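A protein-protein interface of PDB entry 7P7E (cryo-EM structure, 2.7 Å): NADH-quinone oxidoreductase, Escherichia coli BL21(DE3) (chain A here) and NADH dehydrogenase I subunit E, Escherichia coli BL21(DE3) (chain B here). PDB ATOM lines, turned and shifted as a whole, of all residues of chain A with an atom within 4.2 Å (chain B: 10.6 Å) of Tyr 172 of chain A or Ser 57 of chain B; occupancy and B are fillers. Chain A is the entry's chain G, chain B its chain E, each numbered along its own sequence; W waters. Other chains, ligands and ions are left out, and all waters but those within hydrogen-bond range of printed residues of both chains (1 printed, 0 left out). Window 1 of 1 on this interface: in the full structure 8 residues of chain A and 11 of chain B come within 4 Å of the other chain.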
ATOM      1  N   LYS A 161      -1.942  27.164  13.158  1.00  0.00           N
ATOM      2  CA  LYS A 161      -3.109  26.902  13.980  1.00  0.00           C
ATOM      3  C   LYS A 161      -2.781  26.940  15.468  1.00  0.00           C
ATOM      4  O   LYS A 161      -3.424  27.674  16.222  1.00  0.00           O
ATOM      5  CB  LYS A 161      -3.711  25.550  13.587  1.00  0.00           C
ATOM      6  CG  LYS A 161      -5.003  25.197  14.284  1.00  0.00           C
ATOM      7  CD  LYS A 161      -5.723  24.093  13.530  1.00  0.00           C
ATOM      8  CE  LYS A 161      -6.332  24.625  12.243  1.00  0.00           C
ATOM      9  NZ  LYS A 161      -6.661  23.537  11.285  1.00  0.00           N
ATOM     10  N   THR A 167      -7.139  30.004  11.410  1.00  0.00           N
ATOM     11  CA  THR A 167      -8.198  29.019  11.272  1.00  0.00           C
ATOM     12  C   THR A 167      -8.364  28.457   9.867  1.00  0.00           C
ATOM     13  O   THR A 167      -9.030  27.428   9.714  1.00  0.00           O
ATOM     14  CB  THR A 167      -9.544  29.614  11.718  1.00  0.00           C
ATOM     15  OG1 THR A 167      -9.854  30.758  10.915  1.00  0.00           O
ATOM     16  CG2 THR A 167      -9.493  30.025  13.180  1.00  0.00           C
ATOM     17  N   LEU A 169      -6.008  27.365   7.613  1.00  0.00           N
ATOM     18  CA  LEU A 169      -5.034  26.405   7.118  1.00  0.00           C
ATOM     19  C   LEU A 169      -5.191  25.094   7.871  1.00  0.00           C
ATOM     20  O   LEU A 169      -5.542  25.076   9.053  1.00  0.00           O
ATOM     21  CB  LEU A 169      -3.598  26.916   7.260  1.00  0.00           C
ATOM     22  CG  LEU A 169      -2.545  26.302   6.336  1.00  0.00           C
ATOM     23  CD1 LEU A 169      -2.579  26.964   4.975  1.00  0.00           C
ATOM     24  CD2 LEU A 169      -1.162  26.405   6.947  1.00  0.00           C
ATOM     25  N   GLY A 170      -4.934  23.997   7.173  1.00  0.00           N
ATOM     26  CA  GLY A 170      -5.118  22.687   7.767  1.00  0.00           C
ATOM     27  C   GLY A 170      -4.525  21.608   6.892  1.00  0.00           C
ATOM     28  O   GLY A 170      -4.036  21.860   5.785  1.00  0.00           O
ATOM     29  N   VAL A 171      -4.570  20.390   7.423  1.00  0.00           N
ATOM     30  CA  VAL A 171      -4.113  19.194   6.730  1.00  0.00           C
ATOM     31  C   VAL A 171      -5.339  18.366   6.368  1.00  0.00           C
ATOM     32  O   VAL A 171      -6.232  18.162   7.199  1.00  0.00           O
ATOM     33  CB  VAL A 171      -3.105  18.398   7.581  1.00  0.00           C
ATOM     34  CG1 VAL A 171      -3.586  18.241   9.019  1.00  0.00           C
ATOM     35  CG2 VAL A 171      -2.801  17.046   6.954  1.00  0.00           C
ATOM     36  N   TYR A 172      -5.400  17.932   5.116  1.00  0.00           N
ATOM     37  CA  TYR A 172      -6.524  17.198   4.566  1.00  0.00           C
ATOM     38  C   TYR A 172      -6.010  15.917   3.935  1.00  0.00           C
ATOM     39  O   TYR A 172      -4.815  15.752   3.685  1.00  0.00           O
ATOM     40  CB  TYR A 172      -7.282  18.041   3.532  1.00  0.00           C
ATOM     41  CG  TYR A 172      -7.362  19.486   3.931  1.00  0.00           C
ATOM     42  CD1 TYR A 172      -8.267  19.907   4.891  1.00  0.00           C
ATOM     43  CD2 TYR A 172      -6.506  20.424   3.376  1.00  0.00           C
ATOM     44  CE1 TYR A 172      -8.333  21.223   5.273  1.00  0.00           C
ATOM     45  CE2 TYR A 172      -6.563  21.738   3.753  1.00  0.00           C
ATOM     46  CZ  TYR A 172      -7.478  22.134   4.702  1.00  0.00           C
ATOM     47  OH  TYR A 172      -7.535  23.447   5.083  1.00  0.00           O
ATOM     48  N   GLY A 173      -6.933  15.001   3.684  1.00  0.00           N
ATOM     49  CA  GLY A 173      -6.571  13.772   3.020  1.00  0.00           C
ATOM     50  C   GLY A 173      -6.032  12.730   3.983  1.00  0.00           C
ATOM     51  O   GLY A 173      -6.304  12.743   5.182  1.00  0.00           O
ATOM     52  N   ALA A 174      -5.223  11.835   3.436  1.00  0.00           N
ATOM     53  CA  ALA A 174      -4.876  10.592   4.096  1.00  0.00           C
ATOM     54  C   ALA A 174      -3.462  10.215   3.675  1.00  0.00           C
ATOM     55  O   ALA A 174      -2.696  11.064   3.212  1.00  0.00           O
ATOM     56  CB  ALA A 174      -5.916   9.503   3.781  1.00  0.00           C
ATOM     57  N   ASN A 177      -1.357  10.976   0.486  1.00  0.00           N
ATOM     58  CA  ASN A 177      -2.029  12.057  -0.213  1.00  0.00           C
ATOM     59  C   ASN A 177      -2.384  13.200   0.733  1.00  0.00           C
ATOM     60  O   ASN A 177      -3.389  13.883   0.531  1.00  0.00           O
ATOM     61  CB  ASN A 177      -3.282  11.526  -0.908  1.00  0.00           C
ATOM     62  CG  ASN A 177      -3.521  12.171  -2.250  1.00  0.00           C
ATOM     63  OD1 ASN A 177      -2.582  12.472  -2.982  1.00  0.00           O
ATOM     64  ND2 ASN A 177      -4.786  12.390  -2.584  1.00  0.00           N
ATOM     65  N   VAL A 178      -1.581  13.401   1.783  1.00  0.00           N
ATOM     66  CA  VAL A 178      -1.814  14.499   2.712  1.00  0.00           C
ATOM     67  C   VAL A 178      -1.594  15.826   2.002  1.00  0.00           C
ATOM     68  O   VAL A 178      -0.597  16.017   1.294  1.00  0.00           O
ATOM     69  CB  VAL A 178      -0.911  14.379   3.952  1.00  0.00           C
ATOM     70  CG1 VAL A 178      -1.531  13.462   4.981  1.00  0.00           C
ATOM     71  CG2 VAL A 178       0.467  13.880   3.567  1.00  0.00           C
ATOM     72  N   TYR A 179      -2.535  16.744   2.181  1.00  0.00           N
ATOM     73  CA  TYR A 179      -2.534  18.037   1.518  1.00  0.00           C
ATOM     74  C   TYR A 179      -2.563  19.121   2.581  1.00  0.00           C
ATOM     75  O   TYR A 179      -3.436  19.118   3.448  1.00  0.00           O
ATOM     76  CB  TYR A 179      -3.746  18.162   0.592  1.00  0.00           C
ATOM     77  CG  TYR A 179      -3.664  19.248  -0.452  1.00  0.00           C
ATOM     78  CD1 TYR A 179      -3.917  20.573  -0.129  1.00  0.00           C
ATOM     79  CD2 TYR A 179      -3.374  18.939  -1.772  1.00  0.00           C
ATOM     80  CE1 TYR A 179      -3.856  21.561  -1.083  1.00  0.00           C
ATOM     81  CE2 TYR A 179      -3.322  19.918  -2.734  1.00  0.00           C
ATOM     82  CZ  TYR A 179      -3.556  21.229  -2.384  1.00  0.00           C
ATOM     83  OH  TYR A 179      -3.498  22.212  -3.340  1.00  0.00           O
ATOM     84  N   GLY A 181      -3.017  23.062   3.266  1.00  0.00           N
ATOM     85  CA  GLY A 181      -3.496  24.268   2.615  1.00  0.00           C
ATOM     86  C   GLY A 181      -4.814  24.729   3.198  1.00  0.00           C
ATOM     87  O   GLY A 181      -5.127  24.455   4.354  1.00  0.00           O
ATOM     88  N   ARG A 182      -5.556  25.449   2.390  1.00  0.00           N
ATOM     89  CA  ARG A 182      -6.863  25.974   2.737  1.00  0.00           C
ATOM     90  C   ARG A 182      -7.954  25.051   2.219  1.00  0.00           C
ATOM     91  O   ARG A 182      -7.733  24.288   1.274  1.00  0.00           O
ATOM     92  CB  ARG A 182      -7.039  27.376   2.144  1.00  0.00           C
ATOM     93  CG  ARG A 182      -6.040  28.400   2.629  1.00  0.00           C
ATOM     94  CD  ARG A 182      -6.457  29.794   2.211  1.00  0.00           C
ATOM     95  NE  ARG A 182      -7.433  30.377   3.124  1.00  0.00           N
ATOM     96  CZ  ARG A 182      -8.682  30.673   2.795  1.00  0.00           C
ATOM     97  NH1 ARG A 182      -9.155  30.430   1.585  1.00  0.00           N
ATOM     98  NH2 ARG A 182      -9.477  31.229   3.703  1.00  0.00           N
ATOM     99  N   PRO A 183      -9.149  25.069   2.824  1.00  0.00           N
ATOM    100  CA  PRO A 183     -10.250  24.256   2.276  1.00  0.00           C
ATOM    101  C   PRO A 183     -10.713  24.704   0.898  1.00  0.00           C
ATOM    102  O   PRO A 183     -11.347  23.911   0.193  1.00  0.00           O
ATOM    103  CB  PRO A 183     -11.364  24.405   3.321  1.00  0.00           C
ATOM    104  CG  PRO A 183     -11.019  25.609   4.098  1.00  0.00           C
ATOM    105  CD  PRO A 183      -9.536  25.743   4.077  1.00  0.00           C
ATOM    106  N   ARG B  23     -16.660  19.757  19.449  1.00  0.00           N
ATOM    107  CA  ARG B  23     -15.897  19.306  18.287  1.00  0.00           C
ATOM    108  C   ARG B  23     -16.054  17.808  18.053  1.00  0.00           C
ATOM    109  O   ARG B  23     -15.967  17.345  16.911  1.00  0.00           O
ATOM    110  CB  ARG B  23     -14.422  19.671  18.472  1.00  0.00           C
ATOM    111  CG  ARG B  23     -13.512  19.308  17.309  1.00  0.00           C
ATOM    112  CD  ARG B  23     -12.065  19.229  17.749  1.00  0.00           C
ATOM    113  NE  ARG B  23     -11.530  20.548  18.058  1.00  0.00           N
ATOM    114  CZ  ARG B  23     -11.048  21.389  17.155  1.00  0.00           C
ATOM    115  NH1 ARG B  23     -10.999  21.072  15.872  1.00  0.00           N
ATOM    116  NH2 ARG B  23     -10.607  22.579  17.548  1.00  0.00           N
ATOM    117  N   SER B  26     -18.267  16.161  15.133  1.00  0.00           N
ATOM    118  CA  SER B  26     -18.017  16.499  13.731  1.00  0.00           C
ATOM    119  C   SER B  26     -18.206  15.300  12.810  1.00  0.00           C
ATOM    120  O   SER B  26     -18.796  15.432  11.729  1.00  0.00           O
ATOM    121  CB  SER B  26     -16.609  17.074  13.578  1.00  0.00           C
ATOM    122  OG  SER B  26     -15.622  16.103  13.873  1.00  0.00           O
ATOM    123  N   LEU B  30     -21.104  15.076   9.918  1.00  0.00           N
ATOM    124  CA  LEU B  30     -20.825  14.753   8.524  1.00  0.00           C
ATOM    125  C   LEU B  30     -21.604  13.524   8.078  1.00  0.00           C
ATOM    126  O   LEU B  30     -22.117  13.481   6.956  1.00  0.00           O
ATOM    127  CB  LEU B  30     -19.326  14.533   8.327  1.00  0.00           C
ATOM    128  CG  LEU B  30     -18.433  15.764   8.450  1.00  0.00           C
ATOM    129  CD1 LEU B  30     -17.018  15.353   8.793  1.00  0.00           C
ATOM    130  CD2 LEU B  30     -18.460  16.565   7.169  1.00  0.00           C
ATOM    131  N   ASP B  42     -19.484  21.176  -0.192  1.00  0.00           N
ATOM    132  CA  ASP B  42     -18.581  22.125   0.460  1.00  0.00           C
ATOM    133  C   ASP B  42     -19.335  23.063   1.399  1.00  0.00           C
ATOM    134  O   ASP B  42     -18.850  23.396   2.496  1.00  0.00           O
ATOM    135  CB  ASP B  42     -17.832  22.926  -0.603  1.00  0.00           C
ATOM    136  CG  ASP B  42     -17.305  22.053  -1.729  1.00  0.00           C
ATOM    137  OD1 ASP B  42     -16.971  20.879  -1.473  1.00  0.00           O
ATOM    138  OD2 ASP B  42     -17.230  22.541  -2.875  1.00  0.00           O
ATOM    139  N   ALA B  44     -21.878  22.205   3.017  1.00  0.00           N
ATOM    140  CA  ALA B  44     -22.086  21.400   4.212  1.00  0.00           C
ATOM    141  C   ALA B  44     -20.904  21.490   5.164  1.00  0.00           C
ATOM    142  O   ALA B  44     -21.107  21.532   6.381  1.00  0.00           O
ATOM    143  CB  ALA B  44     -22.352  19.947   3.832  1.00  0.00           C
ATOM    144  N   ILE B  45     -19.676  21.524   4.635  1.00  0.00           N
ATOM    145  CA  ILE B  45     -18.494  21.693   5.479  1.00  0.00           C
ATOM    146  C   ILE B  45     -18.563  23.019   6.224  1.00  0.00           C
ATOM    147  O   ILE B  45     -18.371  23.078   7.447  1.00  0.00           O
ATOM    148  CB  ILE B  45     -17.208  21.597   4.635  1.00  0.00           C
ATOM    149  CG1 ILE B  45     -17.115  20.244   3.930  1.00  0.00           C
ATOM    150  CG2 ILE B  45     -15.980  21.850   5.496  1.00  0.00           C
ATOM    151  CD1 ILE B  45     -16.992  19.081   4.869  1.00  0.00           C
ATOM    152  N   HIS B  46     -18.885  24.095   5.500  1.00  0.00           N
ATOM    153  CA  HIS B  46     -18.968  25.404   6.149  1.00  0.00           C
ATOM    154  C   HIS B  46     -20.120  25.475   7.153  1.00  0.00           C
ATOM    155  O   HIS B  46     -19.969  26.060   8.231  1.00  0.00           O
ATOM    156  CB  HIS B  46     -19.093  26.506   5.102  1.00  0.00           C
ATOM    157  CG  HIS B  46     -17.775  27.054   4.651  1.00  0.00           C
ATOM    158  ND1 HIS B  46     -17.071  27.987   5.380  1.00  0.00           N
ATOM    159  CD2 HIS B  46     -17.029  26.794   3.551  1.00  0.00           C
ATOM    160  CE1 HIS B  46     -15.949  28.281   4.748  1.00  0.00           C
ATOM    161  NE2 HIS B  46     -15.899  27.571   3.636  1.00  0.00           N
ATOM    162  N   ALA B  47     -21.266  24.869   6.829  1.00  0.00           N
ATOM    163  CA  ALA B  47     -22.420  24.909   7.725  1.00  0.00           C
ATOM    164  C   ALA B  47     -22.171  24.104   8.997  1.00  0.00           C
ATOM    165  O   ALA B  47     -22.544  24.532  10.098  1.00  0.00           O
ATOM    166  CB  ALA B  47     -23.661  24.396   6.996  1.00  0.00           C
ATOM    167  N   ILE B  48     -21.546  22.931   8.866  1.00  0.00           N
ATOM    168  CA  ILE B  48     -21.199  22.124  10.032  1.00  0.00           C
ATOM    169  C   ILE B  48     -20.182  22.856  10.897  1.00  0.00           C
ATOM    170  O   ILE B  48     -20.267  22.834  12.132  1.00  0.00           O
ATOM    171  CB  ILE B  48     -20.689  20.740   9.582  1.00  0.00           C
ATOM    172  CG1 ILE B  48     -21.848  19.879   9.084  1.00  0.00           C
ATOM    173  CG2 ILE B  48     -19.962  20.010  10.704  1.00  0.00           C
ATOM    174  CD1 ILE B  48     -21.411  18.754   8.181  1.00  0.00           C
ATOM    175  N   ALA B  49     -19.224  23.541  10.263  1.00  0.00           N
ATOM    176  CA  ALA B  49     -18.258  24.339  11.011  1.00  0.00           C
ATOM    177  C   ALA B  49     -18.933  25.476  11.771  1.00  0.00           C
ATOM    178  O   ALA B  49     -18.564  25.769  12.913  1.00  0.00           O
ATOM    179  CB  ALA B  49     -17.199  24.889  10.061  1.00  0.00           C
ATOM    180  N   ASP B  50     -19.914  26.134  11.147  1.00  0.00           N
ATOM    181  CA  ASP B  50     -20.634  27.210  11.823  1.00  0.00           C
ATOM    182  C   ASP B  50     -21.462  26.689  12.992  1.00  0.00           C
ATOM    183  O   ASP B  50     -21.546  27.343  14.037  1.00  0.00           O
ATOM    184  CB  ASP B  50     -21.526  27.961  10.836  1.00  0.00           C
ATOM    185  CG  ASP B  50     -20.740  28.633   9.730  1.00  0.00           C
ATOM    186  OD1 ASP B  50     -19.554  28.956   9.953  1.00  0.00           O
ATOM    187  OD2 ASP B  50     -21.308  28.839   8.637  1.00  0.00           O
ATOM    188  N   GLY B  53     -18.975  25.425  15.921  1.00  0.00           N
ATOM    189  CA  GLY B  53     -18.052  26.379  16.499  1.00  0.00           C
ATOM    190  C   GLY B  53     -16.591  26.082  16.258  1.00  0.00           C
ATOM    191  O   GLY B  53     -15.740  26.589  16.993  1.00  0.00           O
ATOM    192  N   ILE B  54     -16.273  25.280  15.253  1.00  0.00           N
ATOM    193  CA  ILE B  54     -14.890  24.942  14.923  1.00  0.00           C
ATOM    194  C   ILE B  54     -14.621  25.458  13.517  1.00  0.00           C
ATOM    195  O   ILE B  54     -15.563  25.706  12.747  1.00  0.00           O
ATOM    196  CB  ILE B  54     -14.624  23.425  15.060  1.00  0.00           C
ATOM    197  CG1 ILE B  54     -15.517  22.622  14.116  1.00  0.00           C
ATOM    198  CG2 ILE B  54     -14.828  22.981  16.499  1.00  0.00           C
ATOM    199  CD1 ILE B  54     -15.352  21.127  14.259  1.00  0.00           C
ATOM    200  N   PRO B  55     -13.354  25.686  13.162  1.00  0.00           N
ATOM    201  CA  PRO B  55     -13.045  26.156  11.806  1.00  0.00           C
ATOM    202  C   PRO B  55     -13.395  25.137  10.734  1.00  0.00           C
ATOM    203  O   PRO B  55     -13.455  23.930  10.979  1.00  0.00           O
ATOM    204  CB  PRO B  55     -11.534  26.401  11.853  1.00  0.00           C
ATOM    205  CG  PRO B  55     -11.247  26.671  13.270  1.00  0.00           C
ATOM    206  CD  PRO B  55     -12.192  25.826  14.058  1.00  0.00           C
ATOM    207  N   ALA B  56     -13.638  25.651   9.525  1.00  0.00           N
ATOM    208  CA  ALA B  56     -13.950  24.795   8.387  1.00  0.00           C
ATOM    209  C   ALA B  56     -12.770  23.935   7.961  1.00  0.00           C
ATOM    210  O   ALA B  56     -12.982  22.873   7.367  1.00  0.00           O
ATOM    211  CB  ALA B  56     -14.427  25.642   7.207  1.00  0.00           C
ATOM    212  N   SER B  57     -11.540  24.370   8.245  1.00  0.00           N
ATOM    213  CA  SER B  57     -10.369  23.568   7.910  1.00  0.00           C
ATOM    214  C   SER B  57     -10.340  22.268   8.705  1.00  0.00           C
ATOM    215  O   SER B  57      -9.985  21.216   8.166  1.00  0.00           O
ATOM    216  CB  SER B  57      -9.095  24.377   8.144  1.00  0.00           C
ATOM    217  OG  SER B  57      -8.984  24.779   9.496  1.00  0.00           O
ATOM    218  N   ASP B  58     -10.723  22.317   9.984  1.00  0.00           N
ATOM    219  CA  ASP B  58     -10.781  21.101  10.793  1.00  0.00           C
ATOM    220  C   ASP B  58     -11.870  20.153  10.302  1.00  0.00           C
ATOM    221  O   ASP B  58     -11.656  18.934  10.245  1.00  0.00           O
ATOM    222  CB  ASP B  58     -11.000  21.461  12.261  1.00  0.00           C
ATOM    223  CG  ASP B  58      -9.888  22.323  12.817  1.00  0.00           C
ATOM    224  OD1 ASP B  58      -8.784  21.789  13.060  1.00  0.00           O
ATOM    225  OD2 ASP B  58     -10.108  23.534  13.005  1.00  0.00           O
ATOM    226  N   VAL B  59     -13.033  20.696   9.932  1.00  0.00           N
ATOM    227  CA  VAL B  59     -14.123  19.877   9.410  1.00  0.00           C
ATOM    228  C   VAL B  59     -13.719  19.226   8.094  1.00  0.00           C
ATOM    229  O   VAL B  59     -13.993  18.044   7.860  1.00  0.00           O
ATOM    230  CB  VAL B  59     -15.401  20.723   9.253  1.00  0.00           C
ATOM    231  CG1 VAL B  59     -16.542  19.886   8.695  1.00  0.00           C
ATOM    232  CG2 VAL B  59     -15.796  21.339  10.577  1.00  0.00           C
ATOM    233  N   GLU B  60     -13.043  19.978   7.222  1.00  0.00           N
ATOM    234  CA  GLU B  60     -12.606  19.422   5.946  1.00  0.00           C
ATOM    235  C   GLU B  60     -11.499  18.390   6.134  1.00  0.00           C
ATOM    236  O   GLU B  60     -11.461  17.383   5.419  1.00  0.00           O
ATOM    237  CB  GLU B  60     -12.156  20.547   5.011  1.00  0.00           C
ATOM    238  CG  GLU B  60     -11.661  20.087   3.643  1.00  0.00           C
ATOM    239  CD  GLU B  60     -12.781  19.709   2.685  1.00  0.00           C
ATOM    240  OE1 GLU B  60     -13.965  19.834   3.053  1.00  0.00           O
ATOM    241  OE2 GLU B  60     -12.474  19.280   1.554  1.00  0.00           O
ATOM    242  N   GLY B  61     -10.598  18.614   7.094  1.00  0.00           N
ATOM    243  CA  GLY B  61      -9.579  17.618   7.385  1.00  0.00           C
ATOM    244  C   GLY B  61     -10.167  16.324   7.911  1.00  0.00           C
ATOM    245  O   GLY B  61      -9.717  15.234   7.546  1.00  0.00           O
ATOM    246  N   VAL B  62     -11.195  16.428   8.754  1.00  0.00           N
ATOM    247  CA  VAL B  62     -11.903  15.239   9.219  1.00  0.00           C
ATOM    248  C   VAL B  62     -12.613  14.550   8.057  1.00  0.00           C
ATOM    249  O   VAL B  62     -12.509  13.332   7.887  1.00  0.00           O
ATOM    250  CB  VAL B  62     -12.879  15.608  10.350  1.00  0.00           C
ATOM    251  CG1 VAL B  62     -13.858  14.480  10.613  1.00  0.00           C
ATOM    252  CG2 VAL B  62     -12.113  15.944  11.613  1.00  0.00           C
ATOM    253  N   ALA B  63     -13.306  15.325   7.217  1.00  0.00           N
ATOM    254  CA  ALA B  63     -14.092  14.748   6.129  1.00  0.00           C
ATOM    255  C   ALA B  63     -13.211  14.054   5.099  1.00  0.00           C
ATOM    256  O   ALA B  63     -13.583  13.004   4.565  1.00  0.00           O
ATOM    257  CB  ALA B  63     -14.937  15.831   5.463  1.00  0.00           C
ATOM    258  N   THR B  64     -12.043  14.619   4.806  1.00  0.00           N
ATOM    259  CA  THR B  64     -11.133  13.999   3.854  1.00  0.00           C
ATOM    260  C   THR B  64     -10.234  12.946   4.487  1.00  0.00           C
ATOM    261  O   THR B  64      -9.594  12.189   3.752  1.00  0.00           O
ATOM    262  CB  THR B  64     -10.273  15.067   3.178  1.00  0.00           C
ATOM    263  OG1 THR B  64      -9.632  15.866   4.176  1.00  0.00           O
ATOM    264  CG2 THR B  64     -11.126  15.960   2.290  1.00  0.00           C
ATOM    265  N   PHE B  65     -10.155  12.878   5.819  1.00  0.00           N
ATOM    266  CA  PHE B  65      -9.404  11.791   6.438  1.00  0.00           C
ATOM    267  C   PHE B  65     -10.153  10.467   6.339  1.00  0.00           C
ATOM    268  O   PHE B  65      -9.559   9.437   6.003  1.00  0.00           O
ATOM    269  CB  PHE B  65      -9.095  12.117   7.898  1.00  0.00           C
ATOM    270  CG  PHE B  65      -8.205  11.107   8.566  1.00  0.00           C
ATOM    271  CD1 PHE B  65      -6.832  11.166   8.407  1.00  0.00           C
ATOM    272  CD2 PHE B  65      -8.740  10.095   9.348  1.00  0.00           C
ATOM    273  CE1 PHE B  65      -6.010  10.240   9.014  1.00  0.00           C
ATOM    274  CE2 PHE B  65      -7.924   9.165   9.952  1.00  0.00           C
ATOM    275  CZ  PHE B  65      -6.557   9.238   9.788  1.00  0.00           C
ATOM    276  N   TYR B  66     -11.450  10.469   6.632  1.00  0.00           N
ATOM    277  CA  TYR B  66     -12.219   9.237   6.736  1.00  0.00           C
ATOM    278  C   TYR B  66     -12.804   8.863   5.382  1.00  0.00           C
ATOM    279  O   TYR B  66     -13.376   9.709   4.689  1.00  0.00           O
ATOM    280  CB  TYR B  66     -13.321   9.383   7.783  1.00  0.00           C
ATOM    281  CG  TYR B  66     -12.770   9.629   9.163  1.00  0.00           C
ATOM    282  CD1 TYR B  66     -12.227   8.595   9.910  1.00  0.00           C
ATOM    283  CD2 TYR B  66     -12.768  10.899   9.709  1.00  0.00           C
ATOM    284  CE1 TYR B  66     -11.710   8.825  11.164  1.00  0.00           C
ATOM    285  CE2 TYR B  66     -12.250  11.139  10.956  1.00  0.00           C
ATOM    286  CZ  TYR B  66     -11.726  10.100  11.681  1.00  0.00           C
ATOM    287  OH  TYR B  66     -11.214  10.343  12.927  1.00  0.00           O
ATOM    288  N   ARG B  71     -16.849  13.223  -0.138  1.00  0.00           N
ATOM    289  CA  ARG B  71     -16.753  14.620  -0.529  1.00  0.00           C
ATOM    290  C   ARG B  71     -16.926  14.809  -2.030  1.00  0.00           C
ATOM    291  O   ARG B  71     -16.697  15.908  -2.542  1.00  0.00           O
ATOM    292  CB  ARG B  71     -15.419  15.201  -0.062  1.00  0.00           C
ATOM    293  CG  ARG B  71     -15.336  15.398   1.439  1.00  0.00           C
ATOM    294  CD  ARG B  71     -16.226  16.535   1.881  1.00  0.00           C
ATOM    295  NE  ARG B  71     -15.683  17.823   1.473  1.00  0.00           N
ATOM    296  CZ  ARG B  71     -16.215  18.599   0.541  1.00  0.00           C
ATOM    297  NH1 ARG B  71     -17.319  18.253  -0.100  1.00  0.00           N
ATOM    298  NH2 ARG B  71     -15.623  19.751   0.240  1.00  0.00           N
HETATM  299  O   HOH W   1     -11.075  27.315   8.460  1.00  0.00           O
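The backbone NH (N) of Tyr 172 of chain A is in hydrogen-bond range of the backbone carbonyl oxygen (O) of Tyr 179 of chain A (2.8 Å).
The backbone NH of Gly 170 of chain A is in hydrogen-bond range of the side-chain hydroxyl of Tyr 172 of chain A, at 3.4 Å.
The side-chain carboxylate of Glu 60 of chain B is in salt-bridge range of the guanidinium group of Arg 71 of chain B, at 3.1 Å.
O of Gly 181 of chain A is in hydrogen-bond range of OH of Tyr 172 of chain A, at 2.7 Å.
The side-chain hydroxyl of Thr 64 of chain B is in hydrogen-bond range of the backbone carbonyl oxygen of Glu 60 of chain B, at 2.7 Å.
The side-chain carboxylate of Asp 58 of chain B lies within salt-bridge range of the guanidinium group of Arg 23 of chain B (3.7 Å).
The side-chain hydroxyl (OG) of Ser 57 of chain B sits at hydrogen-bond distance from the backbone carbonyl oxygen (O) of Thr 167 of chain A (2.7 Å).
OG1 of Thr 64 of chain B sits at hydrogen-bond distance from N of Gly 173 of chain A (2.9 Å).
The side-chain hydroxyl of Ser 57 of chain B lies within hydrogen-bond range of the backbone carbonyl oxygen of Leu 169 of chain A (3.5 Å).
The side-chain carboxylate (OD1) of Asp 58 of chain B is in salt-bridge range of the side-chain amino group (NZ) of Lys 161 of chain A (3.3 Å).
The side-chain hydroxyl of Ser 57 of chain B lies within hydrogen-bond range of the side-chain amino group of Lys 161 of chain A, 3.2 Å away.
Water W1 lies within hydrogen-bond range of O of Thr 167 of chain A (2.4 Å), N of Ser 57 of chain B (3.0 Å) and N of Ala 56 of chain B (3.2 Å).
Of the printed residues of chain B, Thr 167 of chain A touches Pro 55 and Ser 57.
No residue of chain B comes within 4 Å of Gly 170 of chain A.
Of chain B, only Ser 57 (3.3 Å), Glu 60 (3.6 Å), Gly 61 (3.5 Å) and Thr 64 (3.3 Å) come within 4 Å of Tyr 172 of chain A.
No residue of chain B comes within 4 Å of Ala 174 of chain A.
No residue of chain B comes within 4 Å of Val 178 of chain A.
No residue of chain B comes within 4 Å of Gly 181 of chain A.
Of the printed residues of chain A, Pro 55 of chain B touches Thr 167 (3.4 Å).
Printed residues of chain A within 4 Å of Ser 57 of chain B: Lys 161, Thr 167, Leu 169 and Tyr 172.
Printed residues of chain A within 4 Å of Glu 60 of chain B: Tyr 172 (3.6 Å).
Of the printed residues of chain A, Thr 64 of chain B touches Tyr 172 (3.3 Å) and Gly 173 (2.9 Å).
The nearest printed residue of chain A that does not touch Gly 61 of chain B is Gly 173 of chain A (4.8 Å).
Among the printed residues, pairs that only touch across the chains: Tyr 172 of chain A with Thr 64 of chain B, Tyr 172 of chain A with Ser 57 of chain B, Val 171 of chain A with Gly 61 of chain B, Thr 167 of chain A with Pro 55 of chain B, Tyr 172 of chain A with Gly 61 of chain B, Gly 173 of chain A with Phe 65 of chain B and Tyr 172 of chain A with Glu 60 of chain B.
Hydrophobic or aromatic side chains of chain B within 4 Å of the printed part of chain A: Pro 55 and Phe 65.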
